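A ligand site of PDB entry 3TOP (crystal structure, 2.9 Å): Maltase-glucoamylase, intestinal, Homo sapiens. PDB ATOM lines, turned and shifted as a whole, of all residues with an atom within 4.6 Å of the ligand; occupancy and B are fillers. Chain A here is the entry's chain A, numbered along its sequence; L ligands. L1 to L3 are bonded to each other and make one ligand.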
ATOM      1  N   ASP A 206     -13.387  31.679  -5.669  1.00  0.00           N
ATOM      2  CA  ASP A 206     -13.715  30.408  -5.048  1.00  0.00           C
ATOM      3  C   ASP A 206     -12.717  29.341  -5.518  1.00  0.00           C
ATOM      4  O   ASP A 206     -13.021  28.546  -6.422  1.00  0.00           O
ATOM      5  CB  ASP A 206     -15.164  30.051  -5.355  1.00  0.00           C
ATOM      6  CG  ASP A 206     -15.559  28.663  -4.887  1.00  0.00           C
ATOM      7  OD1 ASP A 206     -16.494  28.106  -5.497  1.00  0.00           O
ATOM      8  OD2 ASP A 206     -14.963  28.124  -3.928  1.00  0.00           O
ATOM      9  N   PRO A 208     -10.134  26.323  -4.003  1.00  0.00           N
ATOM     10  CA  PRO A 208      -9.502  25.589  -2.912  1.00  0.00           C
ATOM     11  C   PRO A 208      -8.003  25.933  -2.849  1.00  0.00           C
ATOM     12  O   PRO A 208      -7.341  25.955  -3.900  1.00  0.00           O
ATOM     13  CB  PRO A 208      -9.708  24.120  -3.308  1.00  0.00           C
ATOM     14  CG  PRO A 208     -10.917  24.123  -4.166  1.00  0.00           C
ATOM     15  CD  PRO A 208     -10.980  25.460  -4.848  1.00  0.00           C
ATOM     16  N   TYR A 300     -20.954  18.412   4.857  1.00  0.00           N
ATOM     17  CA  TYR A 300     -21.764  18.687   3.701  1.00  0.00           C
ATOM     18  C   TYR A 300     -22.418  17.345   3.356  1.00  0.00           C
ATOM     19  O   TYR A 300     -21.736  16.384   2.992  1.00  0.00           O
ATOM     20  CB  TYR A 300     -20.872  19.201   2.559  1.00  0.00           C
ATOM     21  CG  TYR A 300     -21.588  19.581   1.278  1.00  0.00           C
ATOM     22  CD1 TYR A 300     -20.971  19.392   0.061  1.00  0.00           C
ATOM     23  CD2 TYR A 300     -22.859  20.142   1.286  1.00  0.00           C
ATOM     24  CE1 TYR A 300     -21.595  19.739  -1.126  1.00  0.00           C
ATOM     25  CE2 TYR A 300     -23.489  20.500   0.095  1.00  0.00           C
ATOM     26  CZ  TYR A 300     -22.845  20.289  -1.108  1.00  0.00           C
ATOM     27  OH  TYR A 300     -23.436  20.637  -2.299  1.00  0.00           O
ATOM     28  N   ASP A 328     -25.109  21.881   7.091  1.00  0.00           N
ATOM     29  CA  ASP A 328     -24.735  22.569   5.852  1.00  0.00           C
ATOM     30  C   ASP A 328     -26.003  22.949   5.100  1.00  0.00           C
ATOM     31  O   ASP A 328     -27.087  22.914   5.660  1.00  0.00           O
ATOM     32  CB  ASP A 328     -23.815  21.678   5.003  1.00  0.00           C
ATOM     33  CG  ASP A 328     -22.805  22.480   4.210  1.00  0.00           C
ATOM     34  OD1 ASP A 328     -23.115  23.630   3.854  1.00  0.00           O
ATOM     35  OD2 ASP A 328     -21.703  21.953   3.933  1.00  0.00           O
ATOM     36  N   ILE A 329     -25.874  23.299   3.818  1.00  0.00           N
ATOM     37  CA  ILE A 329     -27.032  23.751   3.050  1.00  0.00           C
ATOM     38  C   ILE A 329     -28.101  22.685   2.892  1.00  0.00           C
ATOM     39  O   ILE A 329     -29.163  22.930   2.315  1.00  0.00           O
ATOM     40  CB  ILE A 329     -26.632  24.234   1.658  1.00  0.00           C
ATOM     41  CG1 ILE A 329     -25.634  23.266   1.013  1.00  0.00           C
ATOM     42  CG2 ILE A 329     -26.084  25.651   1.743  1.00  0.00           C
ATOM     43  CD1 ILE A 329     -25.077  23.755  -0.313  1.00  0.00           C
ATOM     44  N   ILE A 364     -25.347  27.893   8.057  1.00  0.00           N
ATOM     45  CA  ILE A 364     -24.705  28.497   6.899  1.00  0.00           C
ATOM     46  C   ILE A 364     -25.672  29.352   6.108  1.00  0.00           C
ATOM     47  O   ILE A 364     -26.872  29.130   6.120  1.00  0.00           O
ATOM     48  CB  ILE A 364     -24.129  27.411   5.970  1.00  0.00           C
ATOM     49  CG1 ILE A 364     -23.258  28.042   4.885  1.00  0.00           C
ATOM     50  CG2 ILE A 364     -25.256  26.606   5.338  1.00  0.00           C
ATOM     51  CD1 ILE A 364     -22.546  27.037   4.002  1.00  0.00           C
ATOM     52  N   ASP A 366     -25.678  31.447   2.109  1.00  0.00           N
ATOM     53  CA  ASP A 366     -24.972  31.869   0.930  1.00  0.00           C
ATOM     54  C   ASP A 366     -25.555  33.240   0.632  1.00  0.00           C
ATOM     55  O   ASP A 366     -26.596  33.609   1.184  1.00  0.00           O
ATOM     56  CB  ASP A 366     -25.159  30.884  -0.225  1.00  0.00           C
ATOM     57  CG  ASP A 366     -24.683  29.453   0.115  1.00  0.00           C
ATOM     58  OD1 ASP A 366     -23.640  29.279   0.789  1.00  0.00           O
ATOM     59  OD2 ASP A 366     -25.378  28.500  -0.307  1.00  0.00           O
ATOM     60  N   TRP A 404     -25.862  27.219  -5.830  1.00  0.00           N
ATOM     61  CA  TRP A 404     -26.361  25.984  -5.250  1.00  0.00           C
ATOM     62  C   TRP A 404     -27.865  25.726  -5.490  1.00  0.00           C
ATOM     63  O   TRP A 404     -28.275  24.606  -5.802  1.00  0.00           O
ATOM     64  CB  TRP A 404     -26.095  25.922  -3.748  1.00  0.00           C
ATOM     65  CG  TRP A 404     -24.659  25.905  -3.319  1.00  0.00           C
ATOM     66  CD1 TRP A 404     -24.083  26.743  -2.407  1.00  0.00           C
ATOM     67  CD2 TRP A 404     -23.632  25.006  -3.750  1.00  0.00           C
ATOM     68  NE1 TRP A 404     -22.758  26.438  -2.260  1.00  0.00           N
ATOM     69  CE2 TRP A 404     -22.456  25.367  -3.067  1.00  0.00           C
ATOM     70  CE3 TRP A 404     -23.586  23.946  -4.650  1.00  0.00           C
ATOM     71  CZ2 TRP A 404     -21.250  24.692  -3.253  1.00  0.00           C
ATOM     72  CZ3 TRP A 404     -22.391  23.276  -4.828  1.00  0.00           C
ATOM     73  CH2 TRP A 404     -21.242  23.647  -4.138  1.00  0.00           C
ATOM     74  N   TRP A 418     -20.451  17.690 -13.683  1.00  0.00           N
ATOM     75  CA  TRP A 418     -20.619  18.877 -12.850  1.00  0.00           C
ATOM     76  C   TRP A 418     -21.091  20.042 -13.713  1.00  0.00           C
ATOM     77  O   TRP A 418     -21.880  20.879 -13.260  1.00  0.00           O
ATOM     78  CB  TRP A 418     -19.330  19.216 -12.102  1.00  0.00           C
ATOM     79  CG  TRP A 418     -19.521  20.301 -11.060  1.00  0.00           C
ATOM     80  CD1 TRP A 418     -19.838  20.130  -9.744  1.00  0.00           C
ATOM     81  CD2 TRP A 418     -19.387  21.714 -11.267  1.00  0.00           C
ATOM     82  NE1 TRP A 418     -19.920  21.351  -9.109  1.00  0.00           N
ATOM     83  CE2 TRP A 418     -19.641  22.341 -10.028  1.00  0.00           C
ATOM     84  CE3 TRP A 418     -19.090  22.517 -12.374  1.00  0.00           C
ATOM     85  CZ2 TRP A 418     -19.610  23.723  -9.861  1.00  0.00           C
ATOM     86  CZ3 TRP A 418     -19.044  23.892 -12.207  1.00  0.00           C
ATOM     87  CH2 TRP A 418     -19.302  24.482 -10.968  1.00  0.00           C
ATOM     88  N   TRP A 467     -22.640  31.358   9.613  1.00  0.00           N
ATOM     89  CA  TRP A 467     -21.500  31.039   8.780  1.00  0.00           C
ATOM     90  C   TRP A 467     -21.785  31.518   7.355  1.00  0.00           C
ATOM     91  O   TRP A 467     -22.269  30.757   6.533  1.00  0.00           O
ATOM     92  CB  TRP A 467     -21.313  29.514   8.851  1.00  0.00           C
ATOM     93  CG  TRP A 467     -20.380  28.897   7.865  1.00  0.00           C
ATOM     94  CD1 TRP A 467     -19.368  29.498   7.195  1.00  0.00           C
ATOM     95  CD2 TRP A 467     -20.384  27.521   7.450  1.00  0.00           C
ATOM     96  NE1 TRP A 467     -18.737  28.579   6.386  1.00  0.00           N
ATOM     97  CE2 TRP A 467     -19.348  27.365   6.520  1.00  0.00           C
ATOM     98  CE3 TRP A 467     -21.165  26.411   7.782  1.00  0.00           C
ATOM     99  CZ2 TRP A 467     -19.062  26.150   5.914  1.00  0.00           C
ATOM    100  CZ3 TRP A 467     -20.895  25.204   7.175  1.00  0.00           C
ATOM    101  CH2 TRP A 467     -19.850  25.082   6.253  1.00  0.00           C
ATOM    102  N   ASP A 469     -20.840  32.217   3.671  1.00  0.00           N
ATOM    103  CA  ASP A 469     -19.858  31.547   2.829  1.00  0.00           C
ATOM    104  C   ASP A 469     -20.198  31.745   1.358  1.00  0.00           C
ATOM    105  O   ASP A 469     -21.241  32.323   1.031  1.00  0.00           O
ATOM    106  CB  ASP A 469     -19.793  30.067   3.193  1.00  0.00           C
ATOM    107  CG  ASP A 469     -19.635  29.149   1.984  1.00  0.00           C
ATOM    108  OD1 ASP A 469     -20.654  28.607   1.506  1.00  0.00           O
ATOM    109  OD2 ASP A 469     -18.494  28.961   1.535  1.00  0.00           O
ATOM    110  N   MET A 470     -19.315  31.288   0.483  1.00  0.00           N
ATOM    111  CA  MET A 470     -19.567  31.323  -0.942  1.00  0.00           C
ATOM    112  C   MET A 470     -19.650  32.775  -1.415  1.00  0.00           C
ATOM    113  O   MET A 470     -20.122  33.063  -2.511  1.00  0.00           O
ATOM    114  CB  MET A 470     -20.860  30.583  -1.240  1.00  0.00           C
ATOM    115  CG  MET A 470     -20.877  29.864  -2.567  1.00  0.00           C
ATOM    116  SD  MET A 470     -19.698  28.517  -2.538  1.00  0.00           S
ATOM    117  CE  MET A 470     -20.184  27.679  -1.040  1.00  0.00           C
ATOM    118  N   PHE A 476     -21.001  29.796 -10.435  1.00  0.00           N
ATOM    119  CA  PHE A 476     -20.602  28.645 -11.252  1.00  0.00           C
ATOM    120  C   PHE A 476     -20.738  28.912 -12.740  1.00  0.00           C
ATOM    121  O   PHE A 476     -20.654  27.991 -13.545  1.00  0.00           O
ATOM    122  CB  PHE A 476     -21.425  27.403 -10.903  1.00  0.00           C
ATOM    123  CG  PHE A 476     -21.274  26.936  -9.476  1.00  0.00           C
ATOM    124  CD1 PHE A 476     -20.290  27.423  -8.669  1.00  0.00           C
ATOM    125  CD2 PHE A 476     -22.134  25.973  -8.964  1.00  0.00           C
ATOM    126  CE1 PHE A 476     -20.158  26.963  -7.372  1.00  0.00           C
ATOM    127  CE2 PHE A 476     -21.998  25.520  -7.678  1.00  0.00           C
ATOM    128  CZ  PHE A 476     -21.010  26.015  -6.882  1.00  0.00           C
ATOM    129  N   LYS A 509     -15.482  32.531 -12.642  1.00  0.00           N
ATOM    130  CA  LYS A 509     -16.080  32.079 -11.387  1.00  0.00           C
ATOM    131  C   LYS A 509     -16.645  33.173 -10.485  1.00  0.00           C
ATOM    132  O   LYS A 509     -16.520  33.104  -9.270  1.00  0.00           O
ATOM    133  CB  LYS A 509     -15.098  31.188 -10.607  1.00  0.00           C
ATOM    134  CG  LYS A 509     -15.020  29.742 -11.102  1.00  0.00           C
ATOM    135  CD  LYS A 509     -14.795  28.749  -9.953  1.00  0.00           C
ATOM    136  CE  LYS A 509     -13.360  28.223  -9.900  1.00  0.00           C
ATOM    137  NZ  LYS A 509     -13.284  26.726  -9.797  1.00  0.00           N
ATOM    138  N   ARG A 559     -15.957  33.485   4.656  1.00  0.00           N
ATOM    139  CA  ARG A 559     -14.939  32.957   3.757  1.00  0.00           C
ATOM    140  C   ARG A 559     -14.066  34.068   3.118  1.00  0.00           C
ATOM    141  O   ARG A 559     -12.843  34.057   3.277  1.00  0.00           O
ATOM    142  CB  ARG A 559     -15.571  32.069   2.687  1.00  0.00           C
ATOM    143  CG  ARG A 559     -14.568  31.154   2.036  1.00  0.00           C
ATOM    144  CD  ARG A 559     -15.230  30.011   1.357  1.00  0.00           C
ATOM    145  NE  ARG A 559     -15.669  30.347   0.025  1.00  0.00           N
ATOM    146  CZ  ARG A 559     -16.014  29.446  -0.887  1.00  0.00           C
ATOM    147  NH1 ARG A 559     -15.961  28.153  -0.586  1.00  0.00           N
ATOM    148  NH2 ARG A 559     -16.400  29.834  -2.107  1.00  0.00           N
ATOM    149  N   TRP A 572     -12.238  30.584   8.383  1.00  0.00           N
ATOM    150  CA  TRP A 572     -11.776  29.218   8.365  1.00  0.00           C
ATOM    151  C   TRP A 572     -11.058  29.151   7.037  1.00  0.00           C
ATOM    152  O   TRP A 572     -11.380  29.912   6.132  1.00  0.00           O
ATOM    153  CB  TRP A 572     -12.962  28.205   8.488  1.00  0.00           C
ATOM    154  CG  TRP A 572     -13.551  27.726   7.188  1.00  0.00           C
ATOM    155  CD1 TRP A 572     -13.255  26.565   6.515  1.00  0.00           C
ATOM    156  CD2 TRP A 572     -14.537  28.401   6.408  1.00  0.00           C
ATOM    157  NE1 TRP A 572     -14.001  26.492   5.357  1.00  0.00           N
ATOM    158  CE2 TRP A 572     -14.786  27.605   5.262  1.00  0.00           C
ATOM    159  CE3 TRP A 572     -15.224  29.596   6.545  1.00  0.00           C
ATOM    160  CZ2 TRP A 572     -15.688  27.985   4.289  1.00  0.00           C
ATOM    161  CZ3 TRP A 572     -16.102  29.974   5.570  1.00  0.00           C
ATOM    162  CH2 TRP A 572     -16.334  29.165   4.459  1.00  0.00           C
ATOM    163  N   ASP A 575     -11.485  25.136   1.584  1.00  0.00           N
ATOM    164  CA  ASP A 575     -11.566  23.779   1.025  1.00  0.00           C
ATOM    165  C   ASP A 575     -10.247  23.002   0.920  1.00  0.00           C
ATOM    166  O   ASP A 575      -9.784  22.659  -0.183  1.00  0.00           O
ATOM    167  CB  ASP A 575     -12.257  23.834  -0.347  1.00  0.00           C
ATOM    168  CG  ASP A 575     -13.667  24.425  -0.245  1.00  0.00           C
ATOM    169  OD1 ASP A 575     -14.275  24.289   0.829  1.00  0.00           O
ATOM    170  OD2 ASP A 575     -14.155  25.031  -1.234  1.00  0.00           O
ATOM    171  N   THR A 577      -7.860  19.556   1.478  1.00  0.00           N
ATOM    172  CA  THR A 577      -8.088  18.169   1.114  1.00  0.00           C
ATOM    173  C   THR A 577      -7.528  17.293   2.221  1.00  0.00           C
ATOM    174  O   THR A 577      -6.643  17.719   2.947  1.00  0.00           O
ATOM    175  CB  THR A 577      -7.439  17.793  -0.240  1.00  0.00           C
ATOM    176  OG1 THR A 577      -8.293  18.223  -1.313  1.00  0.00           O
ATOM    177  CG2 THR A 577      -7.245  16.297  -0.363  1.00  0.00           C
ATOM    178  N   PHE A 608     -11.534  18.602   4.394  1.00  0.00           N
ATOM    179  CA  PHE A 608     -12.769  18.718   3.640  1.00  0.00           C
ATOM    180  C   PHE A 608     -12.814  17.725   2.481  1.00  0.00           C
ATOM    181  O   PHE A 608     -13.331  16.619   2.610  1.00  0.00           O
ATOM    182  CB  PHE A 608     -12.928  20.156   3.165  1.00  0.00           C
ATOM    183  CG  PHE A 608     -14.238  20.429   2.512  1.00  0.00           C
ATOM    184  CD1 PHE A 608     -15.314  20.850   3.268  1.00  0.00           C
ATOM    185  CD2 PHE A 608     -14.387  20.282   1.153  1.00  0.00           C
ATOM    186  CE1 PHE A 608     -16.523  21.116   2.667  1.00  0.00           C
ATOM    187  CE2 PHE A 608     -15.595  20.564   0.546  1.00  0.00           C
ATOM    188  CZ  PHE A 608     -16.668  20.977   1.298  1.00  0.00           C
ATOM    189  N   PHE A 609     -12.246  18.129   1.354  1.00  0.00           N
ATOM    190  CA  PHE A 609     -12.226  17.302   0.155  1.00  0.00           C
ATOM    191  C   PHE A 609     -11.575  15.944   0.388  1.00  0.00           C
ATOM    192  O   PHE A 609     -10.528  15.841   1.004  1.00  0.00           O
ATOM    193  CB  PHE A 609     -11.493  18.011  -0.984  1.00  0.00           C
ATOM    194  CG  PHE A 609     -12.254  19.137  -1.596  1.00  0.00           C
ATOM    195  CD1 PHE A 609     -13.513  18.942  -2.114  1.00  0.00           C
ATOM    196  CD2 PHE A 609     -11.707  20.405  -1.653  1.00  0.00           C
ATOM    197  CE1 PHE A 609     -14.207  19.985  -2.686  1.00  0.00           C
ATOM    198  CE2 PHE A 609     -12.398  21.439  -2.229  1.00  0.00           C
ATOM    199  CZ  PHE A 609     -13.649  21.233  -2.743  1.00  0.00           C
ATOM    200  N   GLN A 610     -12.227  14.902  -0.126  1.00  0.00           N
ATOM    201  CA  GLN A 610     -11.686  13.553  -0.083  1.00  0.00           C
ATOM    202  C   GLN A 610     -11.893  12.799   1.248  1.00  0.00           C
ATOM    203  O   GLN A 610     -12.242  13.383   2.293  1.00  0.00           O
ATOM    204  CB  GLN A 610     -10.221  13.534  -0.524  1.00  0.00           C
ATOM    205  CG  GLN A 610     -10.083  13.690  -2.029  1.00  0.00           C
ATOM    206  CD  GLN A 610      -8.636  13.842  -2.465  1.00  0.00           C
ATOM    207  OE1 GLN A 610      -7.709  13.599  -1.677  1.00  0.00           O
ATOM    208  NE2 GLN A 610      -8.429  14.245  -3.707  1.00  0.00           N
ATOM    209  N   HIS A 633     -15.020  19.467   9.666  1.00  0.00           N
ATOM    210  CA  HIS A 633     -15.950  19.669   8.566  1.00  0.00           C
ATOM    211  C   HIS A 633     -15.466  18.871   7.369  1.00  0.00           C
ATOM    212  O   HIS A 633     -14.315  18.461   7.339  1.00  0.00           O
ATOM    213  CB  HIS A 633     -16.058  21.157   8.227  1.00  0.00           C
ATOM    214  CG  HIS A 633     -16.967  21.467   7.076  1.00  0.00           C
ATOM    215  ND1 HIS A 633     -18.102  20.731   6.806  1.00  0.00           N
ATOM    216  CD2 HIS A 633     -16.917  22.443   6.148  1.00  0.00           C
ATOM    217  CE1 HIS A 633     -18.700  21.234   5.739  1.00  0.00           C
ATOM    218  NE2 HIS A 633     -18.006  22.279   5.320  1.00  0.00           N
ATOM    219  N   THR A 635     -16.563  17.496   3.011  1.00  0.00           N
ATOM    220  CA  THR A 635     -17.381  17.649   1.812  1.00  0.00           C
ATOM    221  C   THR A 635     -18.455  16.565   1.685  1.00  0.00           C
ATOM    222  O   THR A 635     -18.604  15.728   2.562  1.00  0.00           O
ATOM    223  CB  THR A 635     -16.507  17.659   0.553  1.00  0.00           C
ATOM    224  OG1 THR A 635     -17.326  17.930  -0.600  1.00  0.00           O
ATOM    225  CG2 THR A 635     -15.808  16.330   0.382  1.00  0.00           C
HETATM  226  C1  LIG L   1      -9.956  19.509  -5.310  1.00  0.00           C
HETATM  227  C2  LIG L   1     -11.441  19.122  -5.480  1.00  0.00           C
HETATM  228  C3  LIG L   1     -12.329  19.648  -6.617  1.00  0.00           C
HETATM  229  C4  LIG L   1     -11.879  20.988  -6.987  1.00  0.00           C
HETATM  230  C5  LIG L   1     -10.356  20.856  -7.277  1.00  0.00           C
HETATM  231  C6  LIG L   1      -9.754  22.253  -7.739  1.00  0.00           C
HETATM  232  O1  LIG L   1      -9.186  18.383  -5.094  1.00  0.00           O
HETATM  233  O2  LIG L   1     -11.510  17.630  -5.539  1.00  0.00           O
HETATM  234  O3  LIG L   1     -13.665  19.617  -6.261  1.00  0.00           O
HETATM  235  O4  LIG L   1     -12.473  21.356  -8.193  1.00  0.00           O
HETATM  236  O5  LIG L   1      -9.424  20.253  -6.358  1.00  0.00           O
HETATM  237  O6  LIG L   1      -9.390  22.159  -9.087  1.00  0.00           O
HETATM  238  C1  LG2 L   2     -13.656  22.130  -8.147  1.00  0.00           C
HETATM  239  C2  LG2 L   2     -13.461  23.460  -7.490  1.00  0.00           C
HETATM  240  C3  LG2 L   2     -14.469  23.879  -6.436  1.00  0.00           C
HETATM  241  C4  LG2 L   2     -15.655  22.971  -6.284  1.00  0.00           C
HETATM  242  C5  LG2 L   2     -15.291  21.562  -6.542  1.00  0.00           C
HETATM  243  C6  LG2 L   2     -16.534  20.738  -6.553  1.00  0.00           C
HETATM  244  O1  LG2 L   2     -12.199  23.554  -6.942  1.00  0.00           O
HETATM  245  O2  LG2 L   2     -14.868  25.149  -6.760  1.00  0.00           O
HETATM  246  O3  LG2 L   2     -16.071  23.074  -4.941  1.00  0.00           O
HETATM  247  O4  LG2 L   2     -14.744  21.355  -7.790  1.00  0.00           O
HETATM  248  O5  LG2 L   2     -16.547  20.010  -5.383  1.00  0.00           O
HETATM  249  C1  LG3 L   3     -17.429  23.378  -4.811  1.00  0.00           C
HETATM  250  O1  LG3 L   3     -16.864  25.573  -5.453  1.00  0.00           O
HETATM  251  C2  LG3 L   3     -17.516  24.844  -4.505  1.00  0.00           C
HETATM  252  C3  LG3 L   3     -19.176  24.417   2.330  1.00  0.00           C
HETATM  253  C4  LG3 L   3     -16.826  25.112  -3.195  1.00  0.00           C
HETATM  254  O2  LG3 L   3     -16.827  26.564  -2.938  1.00  0.00           O
HETATM  255  C5  LG3 L   3     -17.505  24.310  -2.155  1.00  0.00           C
HETATM  256  N1  LG3 L   3     -17.009  24.588  -0.814  1.00  0.00           N
HETATM  257  C6  LG3 L   3     -17.314  22.890  -2.543  1.00  0.00           C
HETATM  258  O3  LG3 L   3     -17.973  22.623  -3.749  1.00  0.00           O
HETATM  259  C7  LG3 L   3     -17.900  22.029  -1.489  1.00  0.00           C
HETATM  260  C8  LG3 L   3     -17.991  25.457  -0.133  1.00  0.00           C
HETATM  261  C9  LG3 L   3     -17.507  25.828   1.250  1.00  0.00           C
HETATM  262  O4  LG3 L   3     -16.174  26.143   1.219  1.00  0.00           O
HETATM  263  C10 LG3 L   3     -17.728  24.627   2.153  1.00  0.00           C
HETATM  264  O5  LG3 L   3     -17.143  24.846   3.377  1.00  0.00           O
HETATM  265  O6  LG3 L   3     -19.289  23.297   3.114  1.00  0.00           O
HETATM  266  C11 LG3 L   3     -19.831  24.212   1.015  1.00  0.00           C
HETATM  267  C12 LG3 L   3     -19.321  24.797  -0.107  1.00  0.00           C
HETATM  268  C13 LG3 L   3     -21.297  23.906   1.011  1.00  0.00           C
HETATM  269  O7  LG3 L   3     -21.982  25.111   1.091  1.00  0.00           O
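The guanidinium group of Arg 559 lies within salt-bridge range of the side-chain carboxylate of Asp 206 (2.9 Å). The side-chain carboxylate of Asp 575 lies within salt-bridge range of the guanidinium group of Arg 559. The guanidinium group (NH2) of Arg 559 lies within hydrogen-bond range of the side-chain sulfur (SD) of Met 470 (3.6 Å). The guanidinium group (NH1) of Arg 559 is in salt-bridge range of the side-chain carboxylate (OD2) of Asp 469 (3.4 Å). SD of Met 470 sits close to NE1 of Trp 404. The backbone NH (N) of Thr 635 lies close to the backbone carbonyl oxygen (O) of Phe 608 (3.4 Å).
Residues that only touch the ligand: Pro 208, Ile 329, Ile 364, Trp 404, Trp 467, Asp 469, Lys 509, Trp 572, Thr 577, Phe 608 and Phe 609. Hydrophobic or aromatic side chains within 4 Å of the ligand: Pro 208, Ile 329, Ile 364, Trp 404, Trp 467, Met 470, Trp 572, Phe 608, Phe 609 and His 633. Within 4 Å of the ligand: Asp 206, Pro 208, Asp 328, Ile 329, Ile 364, Trp 404, Trp 467, Asp 469, Met 470, Lys 509, Arg 559, Trp 572, Asp 575, Thr 577, Phe 608, Phe 609 and His 633.
O1 of LG3 L3 lies within hydrogen-bond range of OD1 of Asp 206 (2.6 Å). OD2 of Asp 575 lies within salt-bridge range of N1 of LG3 L3, at 2.9 Å. The guanidinium group (NH1) of Arg 559 is in hydrogen-bond range of an oxygen (O4) of LG3 L3 (2.7 Å). An oxygen (O6) of LG3 L3 sits at hydrogen-bond distance from a ring nitrogen (NE2) of His 633, 2.7 Å away. O6 of LG3 L3 lies within hydrogen-bond range of OD2 of Asp 328, at 2.9 Å. The side-chain sulfur (SD) of Met 470 lies within hydrogen-bond range of an oxygen (O2) of LG3 L3, at 3.5 Å.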
